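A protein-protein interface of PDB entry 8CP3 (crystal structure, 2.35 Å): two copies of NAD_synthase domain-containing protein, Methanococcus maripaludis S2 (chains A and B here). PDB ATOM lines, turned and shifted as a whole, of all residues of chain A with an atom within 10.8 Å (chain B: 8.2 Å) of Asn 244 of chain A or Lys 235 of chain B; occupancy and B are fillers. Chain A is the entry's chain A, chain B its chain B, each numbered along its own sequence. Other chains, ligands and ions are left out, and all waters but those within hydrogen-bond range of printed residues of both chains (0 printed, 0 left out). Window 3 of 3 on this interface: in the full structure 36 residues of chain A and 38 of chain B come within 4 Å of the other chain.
Among the printed residues, merely in contact across the chains: Asn 244 of chain A with Ser 238 of chain B (3.4 Å), Asn 251 of chain A with Leu 266 of chain B (3.4 Å), Ile 247 of chain A with Phe 268 of chain B (3.5 Å), Asn 244 of chain A with Lys 235 of chain B (3.6 Å), Phe 242 of chain A with Phe 242 of chain B (3.7 Å) and Ile 247 of chain A with Leu 266 of chain B (3.96 Å).
Asn 244 of chain A touches just these residues of chain B: Lys 235 and Ser 238. Lys 235 of chain B touches just one residue of chain A: Asn 244. Thr 234 of chain B touches none of the printed residues of chain A. Asn 236 of chain B touches none of the printed residues of chain A. Ser 238 of chain B touches one residue of chain A. Phe 268 of chain B touches just one residue of chain A: Ile 247 (3.5 Å). Of the printed residues of chain B, Phe 242 of chain A touches Phe 242. Printed residues of chain B within 4 Å of Ile 247 of chain A: Leu 266 and Phe 268. Of the printed residues of chain A, Leu 266 of chain B touches Ile 247 (3.96 Å) and Asn 251 (3.4 Å). Printed residues of chain A within 4 Å of Phe 242 of chain B: Phe 242. The nearest printed residue of chain B that does not touch Phe 242 of chain A is Ser 238 of chain B (5.3 Å).
Hydrophobic or aromatic side chains of chain B that line the printed part of chain A: Phe 242, Leu 266 and Phe 268. Hydrophobic or aromatic side chains of chain A that line the printed part of chain B: Phe 242 and Ile 247.
Phe 242 of chain B touches its own counterpart, Phe 242 of chain A. Positions printed for both chains: 238, 239, 240, 241 and 242. Of the 6 pairs that touch across the chains among the printed residues, 1 has its exchanged pair printed and touching as well.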
ATOM      1  N   PHE A 214      -9.202  42.668 -28.090  1.00  0.00           N
ATOM      2  CA  PHE A 214      -7.856  42.245 -27.708  1.00  0.00           C
ATOM      3  C   PHE A 214      -6.737  42.998 -28.421  1.00  0.00           C
ATOM      4  O   PHE A 214      -5.574  42.594 -28.323  1.00  0.00           O
ATOM      5  CB  PHE A 214      -7.737  40.734 -27.892  1.00  0.00           C
ATOM      6  CG  PHE A 214      -8.796  39.983 -27.147  1.00  0.00           C
ATOM      7  CD1 PHE A 214     -10.051  39.783 -27.713  1.00  0.00           C
ATOM      8  CD2 PHE A 214      -8.563  39.531 -25.860  1.00  0.00           C
ATOM      9  CE1 PHE A 214     -11.044  39.122 -27.022  1.00  0.00           C
ATOM     10  CE2 PHE A 214      -9.549  38.862 -25.162  1.00  0.00           C
ATOM     11  CZ  PHE A 214     -10.794  38.664 -25.742  1.00  0.00           C
ATOM     12  N   SER A 238      -0.434  36.750 -31.435  1.00  0.00           N
ATOM     13  CA  SER A 238      -0.781  35.575 -30.629  1.00  0.00           C
ATOM     14  C   SER A 238      -0.482  35.783 -29.151  1.00  0.00           C
ATOM     15  O   SER A 238      -1.162  35.204 -28.293  1.00  0.00           O
ATOM     16  CB  SER A 238      -0.046  34.332 -31.140  1.00  0.00           C
ATOM     17  OG  SER A 238       1.313  34.321 -30.729  1.00  0.00           O
ATOM     18  N   GLU A 239       0.529  36.596 -28.835  1.00  0.00           N
ATOM     19  CA  GLU A 239       0.881  36.834 -27.442  1.00  0.00           C
ATOM     20  C   GLU A 239      -0.289  37.420 -26.661  1.00  0.00           C
ATOM     21  O   GLU A 239      -0.379  37.229 -25.444  1.00  0.00           O
ATOM     22  CB  GLU A 239       2.091  37.766 -27.363  1.00  0.00           C
ATOM     23  N   LYS A 240      -1.207  38.106 -27.348  1.00  0.00           N
ATOM     24  CA  LYS A 240      -2.267  38.829 -26.657  1.00  0.00           C
ATOM     25  C   LYS A 240      -3.282  37.888 -26.012  1.00  0.00           C
ATOM     26  O   LYS A 240      -3.716  38.127 -24.879  1.00  0.00           O
ATOM     27  CB  LYS A 240      -2.948  39.798 -27.633  1.00  0.00           C
ATOM     28  CG  LYS A 240      -1.957  40.753 -28.299  1.00  0.00           C
ATOM     29  CD  LYS A 240      -2.620  41.896 -29.046  1.00  0.00           C
ATOM     30  CE  LYS A 240      -1.607  42.999 -29.336  1.00  0.00           C
ATOM     31  NZ  LYS A 240      -1.812  43.634 -30.667  1.00  0.00           N
ATOM     32  N   ILE A 241      -3.665  36.810 -26.709  1.00  0.00           N
ATOM     33  CA  ILE A 241      -4.744  35.931 -26.256  1.00  0.00           C
ATOM     34  C   ILE A 241      -4.294  34.798 -25.330  1.00  0.00           C
ATOM     35  O   ILE A 241      -5.145  34.026 -24.866  1.00  0.00           O
ATOM     36  CB  ILE A 241      -5.493  35.338 -27.469  1.00  0.00           C
ATOM     37  N   PHE A 242      -2.992  34.660 -25.058  1.00  0.00           N
ATOM     38  CA  PHE A 242      -2.472  33.442 -24.420  1.00  0.00           C
ATOM     39  C   PHE A 242      -3.050  33.194 -23.023  1.00  0.00           C
ATOM     40  O   PHE A 242      -3.232  32.036 -22.626  1.00  0.00           O
ATOM     41  CB  PHE A 242      -0.946  33.502 -24.355  1.00  0.00           C
ATOM     42  N   ASP A 243      -3.322  34.252 -22.259  1.00  0.00           N
ATOM     43  CA  ASP A 243      -3.828  34.097 -20.896  1.00  0.00           C
ATOM     44  C   ASP A 243      -5.197  33.420 -20.857  1.00  0.00           C
ATOM     45  O   ASP A 243      -6.054  33.670 -21.710  1.00  0.00           O
ATOM     46  CB  ASP A 243      -3.908  35.455 -20.203  1.00  0.00           C
ATOM     47  CG  ASP A 243      -4.824  36.424 -20.914  1.00  0.00           C
ATOM     48  OD1 ASP A 243      -4.406  36.985 -21.950  1.00  0.00           O
ATOM     49  OD2 ASP A 243      -5.969  36.609 -20.445  1.00  0.00           O
ATOM     50  N   ASN A 244      -5.394  32.555 -19.850  1.00  0.00           N
ATOM     51  CA  ASN A 244      -6.643  31.801 -19.714  1.00  0.00           C
ATOM     52  C   ASN A 244      -7.866  32.712 -19.732  1.00  0.00           C
ATOM     53  O   ASN A 244      -8.914  32.341 -20.275  1.00  0.00           O
ATOM     54  CB  ASN A 244      -6.648  30.999 -18.409  1.00  0.00           C
ATOM     55  CG  ASN A 244      -5.652  29.863 -18.404  1.00  0.00           C
ATOM     56  OD1 ASN A 244      -5.238  29.375 -19.453  1.00  0.00           O
ATOM     57  ND2 ASN A 244      -5.278  29.418 -17.210  1.00  0.00           N
ATOM     58  N   ASP A 245      -7.768  33.874 -19.076  1.00  0.00           N
ATOM     59  CA  ASP A 245      -8.856  34.849 -19.045  1.00  0.00           C
ATOM     60  C   ASP A 245      -9.422  35.127 -20.435  1.00  0.00           C
ATOM     61  O   ASP A 245     -10.633  35.007 -20.664  1.00  0.00           O
ATOM     62  CB  ASP A 245      -8.371  36.141 -18.391  1.00  0.00           C
ATOM     63  CG  ASP A 245      -8.107  35.979 -16.908  1.00  0.00           C
ATOM     64  OD1 ASP A 245      -8.666  35.040 -16.305  1.00  0.00           O
ATOM     65  OD2 ASP A 245      -7.339  36.797 -16.348  1.00  0.00           O
ATOM     66  N   SER A 246      -8.551  35.533 -21.368  1.00  0.00           N
ATOM     67  CA  SER A 246      -8.969  35.800 -22.746  1.00  0.00           C
ATOM     68  C   SER A 246      -9.740  34.624 -23.340  1.00  0.00           C
ATOM     69  O   SER A 246     -10.831  34.797 -23.898  1.00  0.00           O
ATOM     70  CB  SER A 246      -7.748  36.133 -23.603  1.00  0.00           C
ATOM     71  N   ILE A 247      -9.178  33.415 -23.234  1.00  0.00           N
ATOM     72  CA  ILE A 247      -9.804  32.244 -23.839  1.00  0.00           C
ATOM     73  C   ILE A 247     -11.174  31.984 -23.222  1.00  0.00           C
ATOM     74  O   ILE A 247     -12.124  31.615 -23.925  1.00  0.00           O
ATOM     75  CB  ILE A 247      -8.883  31.017 -23.715  1.00  0.00           C
ATOM     76  N   GLU A 248     -11.302  32.170 -21.903  1.00  0.00           N
ATOM     77  CA  GLU A 248     -12.594  31.968 -21.249  1.00  0.00           C
ATOM     78  C   GLU A 248     -13.644  32.927 -21.796  1.00  0.00           C
ATOM     79  O   GLU A 248     -14.789  32.528 -22.048  1.00  0.00           O
ATOM     80  CB  GLU A 248     -12.455  32.126 -19.735  1.00  0.00           C
ATOM     81  N   ARG A 249     -13.273  34.200 -21.975  1.00  0.00           N
ATOM     82  CA  ARG A 249     -14.184  35.181 -22.561  1.00  0.00           C
ATOM     83  C   ARG A 249     -14.448  34.884 -24.033  1.00  0.00           C
ATOM     84  O   ARG A 249     -15.591  34.963 -24.496  1.00  0.00           O
ATOM     85  CB  ARG A 249     -13.624  36.589 -22.387  1.00  0.00           C
ATOM     86  N   ILE A 250     -13.396  34.573 -24.795  1.00  0.00           N
ATOM     87  CA  ILE A 250     -13.585  34.336 -26.222  1.00  0.00           C
ATOM     88  C   ILE A 250     -14.391  33.062 -26.454  1.00  0.00           C
ATOM     89  O   ILE A 250     -15.175  32.983 -27.409  1.00  0.00           O
ATOM     90  CB  ILE A 250     -12.226  34.299 -26.946  1.00  0.00           C
ATOM     91  CG1 ILE A 250     -11.546  35.662 -26.857  1.00  0.00           C
ATOM     92  CG2 ILE A 250     -12.391  33.914 -28.410  1.00  0.00           C
ATOM     93  CD1 ILE A 250     -10.194  35.730 -27.533  1.00  0.00           C
ATOM     94  N   ASN A 251     -14.257  32.067 -25.570  1.00  0.00           N
ATOM     95  CA  ASN A 251     -14.974  30.814 -25.778  1.00  0.00           C
ATOM     96  C   ASN A 251     -16.457  30.978 -25.486  1.00  0.00           C
ATOM     97  O   ASN A 251     -17.299  30.398 -26.181  1.00  0.00           O
ATOM     98  CB  ASN A 251     -14.379  29.701 -24.914  1.00  0.00           C
ATOM     99  N   THR A 252     -16.800  31.766 -24.464  1.00  0.00           N
ATOM    100  CA  THR A 252     -18.210  31.975 -24.148  1.00  0.00           C
ATOM    101  C   THR A 252     -18.886  32.884 -25.176  1.00  0.00           C
ATOM    102  O   THR A 252     -20.023  32.621 -25.588  1.00  0.00           O
ATOM    103  CB  THR A 252     -18.362  32.521 -22.720  1.00  0.00           C
ATOM    104  OG1 THR A 252     -19.750  32.705 -22.416  1.00  0.00           O
ATOM    105  CG2 THR A 252     -17.631  33.847 -22.529  1.00  0.00           C
ATOM    106  N   SER B 218      -3.095  15.974 -16.406  1.00  0.00           N
ATOM    107  CA  SER B 218      -4.537  16.075 -16.276  1.00  0.00           C
ATOM    108  C   SER B 218      -5.214  15.656 -17.581  1.00  0.00           C
ATOM    109  O   SER B 218      -4.565  15.309 -18.572  1.00  0.00           O
ATOM    110  CB  SER B 218      -4.932  17.497 -15.881  1.00  0.00           C
ATOM    111  N   TYR B 219      -6.544  15.708 -17.574  1.00  0.00           N
ATOM    112  CA  TYR B 219      -7.335  15.138 -18.658  1.00  0.00           C
ATOM    113  C   TYR B 219      -7.145  15.918 -19.954  1.00  0.00           C
ATOM    114  O   TYR B 219      -7.319  17.140 -19.982  1.00  0.00           O
ATOM    115  CB  TYR B 219      -8.812  15.102 -18.271  1.00  0.00           C
ATOM    116  N   GLU B 232      -8.483  19.011 -26.337  1.00  0.00           N
ATOM    117  CA  GLU B 232      -9.218  19.451 -25.155  1.00  0.00           C
ATOM    118  C   GLU B 232      -8.303  19.329 -23.945  1.00  0.00           C
ATOM    119  O   GLU B 232      -7.447  18.442 -23.902  1.00  0.00           O
ATOM    120  CB  GLU B 232     -10.483  18.617 -24.895  1.00  0.00           C
ATOM    121  CG  GLU B 232     -11.537  18.642 -25.982  1.00  0.00           C
ATOM    122  CD  GLU B 232     -12.817  17.927 -25.554  1.00  0.00           C
ATOM    123  OE1 GLU B 232     -12.870  17.440 -24.403  1.00  0.00           O
ATOM    124  OE2 GLU B 232     -13.768  17.856 -26.364  1.00  0.00           O
ATOM    125  N   LEU B 233      -8.475  20.224 -22.966  1.00  0.00           N
ATOM    126  CA  LEU B 233      -7.668  20.186 -21.744  1.00  0.00           C
ATOM    127  C   LEU B 233      -8.218  21.161 -20.703  1.00  0.00           C
ATOM    128  O   LEU B 233      -9.089  21.989 -20.986  1.00  0.00           O
ATOM    129  CB  LEU B 233      -6.195  20.489 -22.056  1.00  0.00           C
ATOM    130  CG  LEU B 233      -5.860  21.787 -22.808  1.00  0.00           C
ATOM    131  CD1 LEU B 233      -5.783  23.015 -21.900  1.00  0.00           C
ATOM    132  CD2 LEU B 233      -4.567  21.635 -23.592  1.00  0.00           C
ATOM    133  N   THR B 234      -7.686  21.041 -19.480  1.00  0.00           N
ATOM    134  CA  THR B 234      -8.038  21.863 -18.327  1.00  0.00           C
ATOM    135  C   THR B 234      -7.135  23.096 -18.238  1.00  0.00           C
ATOM    136  O   THR B 234      -6.053  23.149 -18.829  1.00  0.00           O
ATOM    137  CB  THR B 234      -7.944  21.049 -17.037  1.00  0.00           C
ATOM    138  N   LYS B 235      -7.569  24.065 -17.423  1.00  0.00           N
ATOM    139  CA  LYS B 235      -6.882  25.354 -17.333  1.00  0.00           C
ATOM    140  C   LYS B 235      -5.452  25.222 -16.814  1.00  0.00           C
ATOM    141  O   LYS B 235      -4.546  25.914 -17.298  1.00  0.00           O
ATOM    142  CB  LYS B 235      -7.687  26.311 -16.454  1.00  0.00           C
ATOM    143  N   ASN B 236      -5.230  24.373 -15.806  1.00  0.00           N
ATOM    144  CA  ASN B 236      -3.915  24.319 -15.167  1.00  0.00           C
ATOM    145  C   ASN B 236      -2.826  23.960 -16.169  1.00  0.00           C
ATOM    146  O   ASN B 236      -1.739  24.553 -16.157  1.00  0.00           O
ATOM    147  CB  ASN B 236      -3.928  23.318 -14.013  1.00  0.00           C
ATOM    148  N   GLU B 237      -3.094  22.983 -17.038  1.00  0.00           N
ATOM    149  CA  GLU B 237      -2.154  22.673 -18.108  1.00  0.00           C
ATOM    150  C   GLU B 237      -2.095  23.795 -19.140  1.00  0.00           C
ATOM    151  O   GLU B 237      -1.060  23.974 -19.796  1.00  0.00           O
ATOM    152  CB  GLU B 237      -2.531  21.346 -18.768  1.00  0.00           C
ATOM    153  N   SER B 238      -3.189  24.556 -19.291  1.00  0.00           N
ATOM    154  CA  SER B 238      -3.312  25.505 -20.401  1.00  0.00           C
ATOM    155  C   SER B 238      -2.215  26.560 -20.396  1.00  0.00           C
ATOM    156  O   SER B 238      -1.804  27.030 -21.464  1.00  0.00           O
ATOM    157  CB  SER B 238      -4.685  26.180 -20.368  1.00  0.00           C
ATOM    158  N   GLU B 239      -1.747  26.968 -19.214  1.00  0.00           N
ATOM    159  CA  GLU B 239      -0.693  27.976 -19.161  1.00  0.00           C
ATOM    160  C   GLU B 239       0.592  27.482 -19.823  1.00  0.00           C
ATOM    161  O   GLU B 239       1.381  28.292 -20.325  1.00  0.00           O
ATOM    162  CB  GLU B 239      -0.428  28.379 -17.712  1.00  0.00           C
ATOM    163  N   LYS B 240       0.808  26.159 -19.846  1.00  0.00           N
ATOM    164  CA  LYS B 240       2.070  25.603 -20.331  1.00  0.00           C
ATOM    165  C   LYS B 240       2.228  25.762 -21.842  1.00  0.00           C
ATOM    166  O   LYS B 240       3.335  26.036 -22.329  1.00  0.00           O
ATOM    167  CB  LYS B 240       2.168  24.127 -19.946  1.00  0.00           C
ATOM    168  N   ILE B 241       1.143  25.580 -22.604  1.00  0.00           N
ATOM    169  CA  ILE B 241       1.246  25.592 -24.061  1.00  0.00           C
ATOM    170  C   ILE B 241       1.258  27.004 -24.627  1.00  0.00           C
ATOM    171  O   ILE B 241       1.552  27.189 -25.817  1.00  0.00           O
ATOM    172  CB  ILE B 241       0.075  24.772 -24.638  1.00  0.00           C
ATOM    173  CG1 ILE B 241       0.176  24.596 -26.157  1.00  0.00           C
ATOM    174  CG2 ILE B 241      -1.257  25.427 -24.297  1.00  0.00           C
ATOM    175  CD1 ILE B 241       1.187  23.570 -26.596  1.00  0.00           C
ATOM    176  N   PHE B 242       1.029  28.018 -23.787  1.00  0.00           N
ATOM    177  CA  PHE B 242       0.839  29.375 -24.291  1.00  0.00           C
ATOM    178  C   PHE B 242       2.071  29.870 -25.034  1.00  0.00           C
ATOM    179  O   PHE B 242       1.946  30.649 -25.988  1.00  0.00           O
ATOM    180  CB  PHE B 242       0.475  30.325 -23.148  1.00  0.00           C
ATOM    181  N   LEU B 266     -11.053  26.113 -26.923  1.00  0.00           N
ATOM    182  CA  LEU B 266     -10.991  27.162 -25.912  1.00  0.00           C
ATOM    183  C   LEU B 266     -11.911  26.882 -24.727  1.00  0.00           C
ATOM    184  O   LEU B 266     -11.925  27.662 -23.766  1.00  0.00           O
ATOM    185  CB  LEU B 266     -11.337  28.516 -26.533  1.00  0.00           C
ATOM    186  N   ASN B 267     -12.687  25.801 -24.790  1.00  0.00           N
ATOM    187  CA  ASN B 267     -13.528  25.332 -23.692  1.00  0.00           C
ATOM    188  C   ASN B 267     -12.657  24.456 -22.797  1.00  0.00           C
ATOM    189  O   ASN B 267     -12.508  23.253 -23.016  1.00  0.00           O
ATOM    190  CB  ASN B 267     -14.730  24.563 -24.243  1.00  0.00           C
ATOM    191  CG  ASN B 267     -15.779  24.239 -23.186  1.00  0.00           C
ATOM    192  OD1 ASN B 267     -15.473  24.101 -22.001  1.00  0.00           O
ATOM    193  ND2 ASN B 267     -17.025  24.084 -23.624  1.00  0.00           N
ATOM    194  N   PHE B 268     -12.064  25.066 -21.774  1.00  0.00           N
ATOM    195  CA  PHE B 268     -11.238  24.322 -20.830  1.00  0.00           C
ATOM    196  C   PHE B 268     -12.137  23.615 -19.821  1.00  0.00           C
ATOM    197  O   PHE B 268     -12.854  24.271 -19.056  1.00  0.00           O
ATOM    198  CB  PHE B 268     -10.261  25.248 -20.113  1.00  0.00           C
ATOM    199  CG  PHE B 268      -9.330  25.972 -21.036  1.00  0.00           C
ATOM    200  CD1 PHE B 268      -8.389  25.279 -21.779  1.00  0.00           C
ATOM    201  CD2 PHE B 268      -9.397  27.349 -21.156  1.00  0.00           C
ATOM    202  CE1 PHE B 268      -7.529  25.948 -22.634  1.00  0.00           C
ATOM    203  CE2 PHE B 268      -8.544  28.023 -22.002  1.00  0.00           C
ATOM    204  CZ  PHE B 268      -7.607  27.323 -22.744  1.00  0.00           C
ATOM    205  N   LYS B 269     -12.085  22.281 -19.810  1.00  0.00           N
ATOM    206  CA  LYS B 269     -12.941  21.495 -18.931  1.00  0.00           C
ATOM    207  C   LYS B 269     -12.690  21.859 -17.468  1.00  0.00           C
ATOM    208  O   LYS B 269     -11.633  22.382 -17.101  1.00  0.00           O
ATOM    209  CB  LYS B 269     -12.711  20.001 -19.157  1.00  0.00           C
ATOM    210  N   GLY B 270     -13.686  21.573 -16.630  1.00  0.00           N
ATOM    211  CA  GLY B 270     -13.708  22.004 -15.237  1.00  0.00           C
ATOM    212  C   GLY B 270     -12.456  21.758 -14.412  1.00  0.00           C
ATOM    213  O   GLY B 270     -11.900  20.659 -14.402  1.00  0.00           O
